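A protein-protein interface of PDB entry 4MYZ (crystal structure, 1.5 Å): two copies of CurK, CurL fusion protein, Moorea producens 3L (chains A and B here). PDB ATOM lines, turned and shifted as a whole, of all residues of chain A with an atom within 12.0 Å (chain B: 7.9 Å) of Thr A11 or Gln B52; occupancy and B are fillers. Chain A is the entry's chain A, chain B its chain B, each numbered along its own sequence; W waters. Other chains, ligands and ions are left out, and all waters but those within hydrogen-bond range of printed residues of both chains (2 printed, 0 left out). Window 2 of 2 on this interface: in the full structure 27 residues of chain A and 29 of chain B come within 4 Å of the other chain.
Water W2 lies within hydrogen-bond range of the backbone carbonyl oxygen (O) of Ile A10, the side-chain amide nitrogen (NE2) of Gln B58 and the backbone carbonyl oxygen (O) of Leu A13.
Water W1 lies within hydrogen-bond range of the side-chain amide nitrogen (NE2) of Gln B52, the side-chain amide nitrogen (NE2) of Gln B58 and the backbone carbonyl oxygen (O) of Thr A11.
No residue of chain A comes within 4 Å of Glu B51.
Leu B54 touches just these residues of chain A: Ile A10 and Thr A11.
Printed residues of chain A within 4 Å of Ile B62: Ile A10.
Of the printed residues of chain A, Gln B58 touches Ile A10, Thr A11 and Leu A18.
Of the printed residues of chain B, Ile A10 touches Leu B54, Gln B58 and Ile B62.
Printed residues of chain B within 4 Å of Leu A18: Gln B58 (3.8 Å).
Ser A21 touches none of the printed residues of chain B.
The nearest residue of chain A that does not touch Gln B52 is Glu A12 (6.5 Å).
No position is printed for both chains.
Among the printed residues, merely in contact across the chains: Ile A10 with Leu B54, Ile A10 with Gln B58, Ile A10 with Ile B62, Thr A11 with Gln B52, Thr A11 with Leu B54, Thr A11 with Gln B58 and Leu A18 with Gln B58.
Of the 13 printed residues of chain A, 3 touch a printed residue of chain B.
Along chain A the printed residues that touch a printed residue of chain B span positions 10 to 18.
Of the 9 printed residues of chain B, 4 touch a printed residue of chain A.
Along chain B the printed residues that touch a printed residue of chain A span positions 52 to 62.
Among the printed residues, 7 pairs touch across the chains.
Among the printed residues, no Asp or Glu carboxylate lies within 4 Å of a Lys or Arg side-chain nitrogen of the other chain.
The backbone NH of Ser B55 is in hydrogen-bond range of the side-chain amide oxygen of Gln B58, at 2.9 Å.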
ATOM      1  N   ASP A   9      26.970 -26.652  14.457  1.00  0.00           N
ATOM      2  CA  ASP A   9      27.777 -25.492  14.949  1.00  0.00           C
ATOM      3  C   ASP A   9      27.359 -24.249  14.170  1.00  0.00           C
ATOM      4  O   ASP A   9      26.866 -24.349  13.048  1.00  0.00           O
ATOM      5  CB  ASP A   9      29.285 -25.743  14.789  1.00  0.00           C
ATOM      6  CG  ASP A   9      29.703 -27.140  15.233  1.00  0.00           C
ATOM      7  OD1 ASP A   9      29.122 -28.125  14.724  1.00  0.00           O
ATOM      8  OD2 ASP A   9      30.623 -27.262  16.075  1.00  0.00           O
ATOM      9  N   ILE A  10      27.540 -23.079  14.768  1.00  0.00           N
ATOM     10  CA  ILE A  10      27.104 -21.833  14.129  1.00  0.00           C
ATOM     11  C   ILE A  10      27.752 -21.623  12.763  1.00  0.00           C
ATOM     12  O   ILE A  10      27.123 -21.062  11.857  1.00  0.00           O
ATOM     13  CB  ILE A  10      27.368 -20.607  15.023  1.00  0.00           C
ATOM     14  CG1 ILE A  10      26.658 -19.383  14.438  1.00  0.00           C
ATOM     15  CG2 ILE A  10      28.871 -20.366  15.178  1.00  0.00           C
ATOM     16  CD1 ILE A  10      26.621 -18.202  15.355  1.00  0.00           C
ATOM     17  N   THR A  11      28.976 -22.093  12.575  1.00  0.00           N
ATOM     18  CA  THR A  11      29.630 -21.915  11.279  1.00  0.00           C
ATOM     19  C   THR A  11      29.066 -22.840  10.217  1.00  0.00           C
ATOM     20  O   THR A  11      29.344 -22.658   9.037  1.00  0.00           O
ATOM     21  CB  THR A  11      31.163 -22.071  11.348  1.00  0.00           C
ATOM     22  OG1 THR A  11      31.499 -23.388  11.799  1.00  0.00           O
ATOM     23  CG2 THR A  11      31.752 -21.035  12.264  1.00  0.00           C
ATOM     24  N   GLU A  12      28.264 -23.818  10.625  1.00  0.00           N
ATOM     25  CA  GLU A  12      27.604 -24.698   9.663  1.00  0.00           C
ATOM     26  C   GLU A  12      26.423 -24.010   8.976  1.00  0.00           C
ATOM     27  O   GLU A  12      25.955 -24.481   7.946  1.00  0.00           O
ATOM     28  CB  GLU A  12      27.102 -25.987  10.336  1.00  0.00           C
ATOM     29  CG  GLU A  12      28.175 -26.834  11.005  1.00  0.00           C
ATOM     30  CD  GLU A  12      28.765 -27.875  10.080  1.00  0.00           C
ATOM     31  OE1 GLU A  12      29.110 -27.521   8.932  1.00  0.00           O
ATOM     32  OE2 GLU A  12      28.896 -29.050  10.507  1.00  0.00           O
ATOM     33  N   LEU A  13      25.922 -22.921   9.552  1.00  0.00           N
ATOM     34  CA  LEU A  13      24.744 -22.234   8.986  1.00  0.00           C
ATOM     35  C   LEU A  13      25.125 -21.478   7.712  1.00  0.00           C
ATOM     36  O   LEU A  13      26.124 -20.751   7.694  1.00  0.00           O
ATOM     37  CB  LEU A  13      24.116 -21.256   9.982  1.00  0.00           C
ATOM     38  CG  LEU A  13      23.543 -21.751  11.306  1.00  0.00           C
ATOM     39  CD1 LEU A  13      23.006 -20.605  12.148  1.00  0.00           C
ATOM     40  CD2 LEU A  13      22.453 -22.776  11.043  1.00  0.00           C
ATOM     41  N   SER A  14      24.300 -21.592   6.669  1.00  0.00           N
ATOM     42  CA  SER A  14      24.443 -20.756   5.493  1.00  0.00           C
ATOM     43  C   SER A  14      24.150 -19.290   5.857  1.00  0.00           C
ATOM     44  O   SER A  14      23.558 -19.013   6.896  1.00  0.00           O
ATOM     45  CB  SER A  14      23.479 -21.204   4.382  1.00  0.00           C
ATOM     46  OG  SER A  14      22.128 -20.849   4.698  1.00  0.00           O
ATOM     47  N   GLU A  15      24.488 -18.361   4.970  1.00  0.00           N
ATOM     48  CA  GLU A  15      24.196 -16.977   5.241  1.00  0.00           C
ATOM     49  C   GLU A  15      22.701 -16.729   5.430  1.00  0.00           C
ATOM     50  O   GLU A  15      22.292 -15.997   6.341  1.00  0.00           O
ATOM     51  CB  GLU A  15      24.715 -16.064   4.154  1.00  0.00           C
ATOM     52  CG  GLU A  15      24.878 -14.653   4.656  1.00  0.00           C
ATOM     53  CD  GLU A  15      26.153 -14.492   5.567  1.00  0.00           C
ATOM     54  OE1 GLU A  15      27.025 -15.378   5.598  1.00  0.00           O
ATOM     55  OE2 GLU A  15      26.224 -13.532   6.323  1.00  0.00           O
ATOM     56  N   ILE A  16      21.863 -17.366   4.617  1.00  0.00           N
ATOM     57  CA  ILE A  16      20.418 -17.236   4.758  1.00  0.00           C
ATOM     58  C   ILE A  16      19.947 -17.805   6.092  1.00  0.00           C
ATOM     59  O   ILE A  16      19.109 -17.199   6.775  1.00  0.00           O
ATOM     60  CB  ILE A  16      19.677 -17.849   3.562  1.00  0.00           C
ATOM     61  CG1 ILE A  16      19.866 -16.962   2.329  1.00  0.00           C
ATOM     62  CG2 ILE A  16      18.207 -17.953   3.861  1.00  0.00           C
ATOM     63  CD1 ILE A  16      19.479 -17.628   1.021  1.00  0.00           C
ATOM     64  N   GLU A  17      20.440 -18.978   6.460  1.00  0.00           N
ATOM     65  CA  GLU A  17      20.063 -19.555   7.742  1.00  0.00           C
ATOM     66  C   GLU A  17      20.496 -18.664   8.900  1.00  0.00           C
ATOM     67  O   GLU A  17      19.748 -18.525   9.886  1.00  0.00           O
ATOM     68  CB  GLU A  17      20.613 -20.983   7.901  1.00  0.00           C
ATOM     69  CG  GLU A  17      20.084 -21.975   6.881  1.00  0.00           C
ATOM     70  CD  GLU A  17      20.867 -23.274   6.816  1.00  0.00           C
ATOM     71  OE1 GLU A  17      21.973 -23.369   7.419  1.00  0.00           O
ATOM     72  OE2 GLU A  17      20.370 -24.226   6.166  1.00  0.00           O
ATOM     73  N   LEU A  18      21.684 -18.066   8.797  1.00  0.00           N
ATOM     74  CA  LEU A  18      22.162 -17.142   9.831  1.00  0.00           C
ATOM     75  C   LEU A  18      21.228 -15.929   9.937  1.00  0.00           C
ATOM     76  O   LEU A  18      20.803 -15.548  11.025  1.00  0.00           O
ATOM     77  CB  LEU A  18      23.575 -16.712   9.496  1.00  0.00           C
ATOM     78  CG  LEU A  18      24.253 -15.731  10.386  1.00  0.00           C
ATOM     79  CD1 LEU A  18      24.358 -16.263  11.816  1.00  0.00           C
ATOM     80  CD2 LEU A  18      25.628 -15.479   9.813  1.00  0.00           C
ATOM     81  N   GLU A  19      20.917 -15.301   8.806  1.00  0.00           N
ATOM     82  CA  GLU A  19      20.002 -14.165   8.844  1.00  0.00           C
ATOM     83  C   GLU A  19      18.630 -14.526   9.413  1.00  0.00           C
ATOM     84  O   GLU A  19      18.074 -13.800  10.222  1.00  0.00           O
ATOM     85  CB  GLU A  19      19.851 -13.547   7.456  1.00  0.00           C
ATOM     86  CG  GLU A  19      21.142 -12.915   6.927  1.00  0.00           C
ATOM     87  CD  GLU A  19      20.987 -12.312   5.558  1.00  0.00           C
ATOM     88  OE1 GLU A  19      19.833 -12.132   5.102  1.00  0.00           O
ATOM     89  OE2 GLU A  19      22.024 -12.031   4.910  1.00  0.00           O
ATOM     90  N   SER A  21      17.930 -16.923  11.469  1.00  0.00           N
ATOM     91  CA  SER A  21      18.092 -17.180  12.901  1.00  0.00           C
ATOM     92  C   SER A  21      18.194 -15.894  13.688  1.00  0.00           C
ATOM     93  O   SER A  21      17.639 -15.777  14.786  1.00  0.00           O
ATOM     94  CB  SER A  21      19.320 -18.045  13.130  1.00  0.00           C
ATOM     95  OG  SER A  21      19.123 -19.340  12.588  1.00  0.00           O
ATOM     96  N   VAL A  22      18.931 -14.931  13.162  1.00  0.00           N
ATOM     97  CA  VAL A  22      19.066 -13.628  13.814  1.00  0.00           C
ATOM     98  C   VAL A  22      17.698 -12.952  13.918  1.00  0.00           C
ATOM     99  O   VAL A  22      17.330 -12.474  14.986  1.00  0.00           O
ATOM    100  CB  VAL A  22      20.094 -12.757  13.078  1.00  0.00           C
ATOM    101  CG1 VAL A  22      19.957 -11.297  13.478  1.00  0.00           C
ATOM    102  CG2 VAL A  22      21.500 -13.265  13.269  1.00  0.00           C
ATOM    103  N   LYS B  50      37.586 -27.069  10.151  1.00  0.00           N
ATOM    104  CA  LYS B  50      37.500 -27.129  11.608  1.00  0.00           C
ATOM    105  C   LYS B  50      37.449 -25.720  12.216  1.00  0.00           C
ATOM    106  O   LYS B  50      36.379 -25.119  12.314  1.00  0.00           O
ATOM    107  CB  LYS B  50      38.693 -27.911  12.183  1.00  0.00           C
ATOM    108  CG  LYS B  50      38.627 -29.423  12.040  1.00  0.00           C
ATOM    109  CD  LYS B  50      39.965 -30.030  12.441  1.00  0.00           C
ATOM    110  CE  LYS B  50      39.948 -31.548  12.419  1.00  0.00           C
ATOM    111  NZ  LYS B  50      39.341 -32.119  13.653  1.00  0.00           N
ATOM    112  N   GLU B  51      38.611 -25.201  12.613  1.00  0.00           N
ATOM    113  CA  GLU B  51      38.717 -23.897  13.265  1.00  0.00           C
ATOM    114  C   GLU B  51      38.261 -22.843  12.275  1.00  0.00           C
ATOM    115  O   GLU B  51      38.644 -22.903  11.109  1.00  0.00           O
ATOM    116  CB  GLU B  51      40.180 -23.645  13.676  1.00  0.00           C
ATOM    117  CG  GLU B  51      40.401 -22.396  14.506  1.00  0.00           C
ATOM    118  CD  GLU B  51      41.865 -22.132  14.810  1.00  0.00           C
ATOM    119  OE1 GLU B  51      42.708 -23.029  14.604  1.00  0.00           O
ATOM    120  OE2 GLU B  51      42.168 -21.013  15.275  1.00  0.00           O
ATOM    121  N   GLN B  52      37.435 -21.899  12.726  1.00  0.00           N
ATOM    122  CA  GLN B  52      36.963 -20.807  11.871  1.00  0.00           C
ATOM    123  C   GLN B  52      36.637 -19.574  12.705  1.00  0.00           C
ATOM    124  O   GLN B  52      35.775 -19.637  13.574  1.00  0.00           O
ATOM    125  CB  GLN B  52      35.712 -21.231  11.074  1.00  0.00           C
ATOM    126  CG  GLN B  52      35.208 -20.141  10.124  1.00  0.00           C
ATOM    127  CD  GLN B  52      34.122 -20.619   9.161  1.00  0.00           C
ATOM    128  OE1 GLN B  52      34.124 -21.773   8.710  1.00  0.00           O
ATOM    129  NE2 GLN B  52      33.200 -19.729   8.830  1.00  0.00           N
ATOM    130  N   SER B  53      37.260 -18.439  12.389  1.00  0.00           N
ATOM    131  CA  SER B  53      36.996 -17.176  13.056  1.00  0.00           C
ATOM    132  C   SER B  53      35.594 -16.687  12.696  1.00  0.00           C
ATOM    133  O   SER B  53      35.204 -16.726  11.544  1.00  0.00           O
ATOM    134  CB  SER B  53      37.969 -16.097  12.619  1.00  0.00           C
ATOM    135  OG  SER B  53      39.234 -16.359  13.174  1.00  0.00           O
ATOM    136  N   LEU B  54      34.867 -16.205  13.687  1.00  0.00           N
ATOM    137  CA  LEU B  54      33.454 -15.836  13.500  1.00  0.00           C
ATOM    138  C   LEU B  54      33.320 -14.445  12.919  1.00  0.00           C
ATOM    139  O   LEU B  54      34.116 -13.527  13.239  1.00  0.00           O
ATOM    140  CB  LEU B  54      32.703 -15.844  14.808  1.00  0.00           C
ATOM    141  CG  LEU B  54      32.659 -17.167  15.546  1.00  0.00           C
ATOM    142  CD1 LEU B  54      31.797 -17.038  16.799  1.00  0.00           C
ATOM    143  CD2 LEU B  54      32.162 -18.255  14.634  1.00  0.00           C
ATOM    144  N   SER B  55      32.312 -14.263  12.081  1.00  0.00           N
ATOM    145  CA  SER B  55      31.977 -12.936  11.602  1.00  0.00           C
ATOM    146  C   SER B  55      31.119 -12.181  12.621  1.00  0.00           C
ATOM    147  O   SER B  55      30.569 -12.784  13.558  1.00  0.00           O
ATOM    148  CB  SER B  55      31.185 -13.069  10.311  1.00  0.00           C
ATOM    149  OG  SER B  55      29.918 -13.667  10.547  1.00  0.00           O
ATOM    150  N   GLN B  58      27.641 -13.686  12.938  1.00  0.00           N
ATOM    151  CA  GLN B  58      27.669 -14.929  13.726  1.00  0.00           C
ATOM    152  C   GLN B  58      27.757 -14.605  15.204  1.00  0.00           C
ATOM    153  O   GLN B  58      27.046 -15.211  16.027  1.00  0.00           O
ATOM    154  CB  GLN B  58      28.840 -15.814  13.307  1.00  0.00           C
ATOM    155  CG  GLN B  58      28.589 -16.516  11.963  1.00  0.00           C
ATOM    156  CD  GLN B  58      29.822 -17.194  11.399  1.00  0.00           C
ATOM    157  OE1 GLN B  58      30.939 -16.745  11.565  1.00  0.00           O
ATOM    158  NE2 GLN B  58      29.578 -18.239  10.596  1.00  0.00           N
ATOM    159  N   ARG B  59      28.675 -13.702  15.565  1.00  0.00           N
ATOM    160  CA  ARG B  59      28.757 -13.299  16.961  1.00  0.00           C
ATOM    161  C   ARG B  59      27.460 -12.655  17.455  1.00  0.00           C
ATOM    162  O   ARG B  59      27.074 -12.823  18.612  1.00  0.00           O
ATOM    163  CB  ARG B  59      29.947 -12.389  17.224  1.00  0.00           C
ATOM    164  CG  ARG B  59      31.297 -13.018  17.021  1.00  0.00           C
ATOM    165  CD  ARG B  59      32.325 -12.189  17.755  1.00  0.00           C
ATOM    166  NE  ARG B  59      33.703 -12.648  17.623  1.00  0.00           N
ATOM    167  CZ  ARG B  59      34.270 -13.569  18.380  1.00  0.00           C
ATOM    168  NH1 ARG B  59      33.578 -14.223  19.298  1.00  0.00           N
ATOM    169  NH2 ARG B  59      35.567 -13.824  18.218  1.00  0.00           N
ATOM    170  N   ILE B  62      24.939 -15.306  18.492  1.00  0.00           N
ATOM    171  CA  ILE B  62      25.279 -15.875  19.819  1.00  0.00           C
ATOM    172  C   ILE B  62      24.881 -14.881  20.927  1.00  0.00           C
ATOM    173  O   ILE B  62      24.267 -15.275  21.927  1.00  0.00           O
ATOM    174  CB  ILE B  62      26.769 -16.234  19.875  1.00  0.00           C
ATOM    175  CG1 ILE B  62      27.055 -17.407  18.939  1.00  0.00           C
ATOM    176  CG2 ILE B  62      27.207 -16.556  21.283  1.00  0.00           C
ATOM    177  CD1 ILE B  62      28.512 -17.632  18.658  1.00  0.00           C
HETATM  178  O   HOH W   1      30.413 -19.875   8.123  1.00  0.00           O
HETATM  179  O   HOH W   2      27.004 -19.142  10.005  1.00  0.00           O
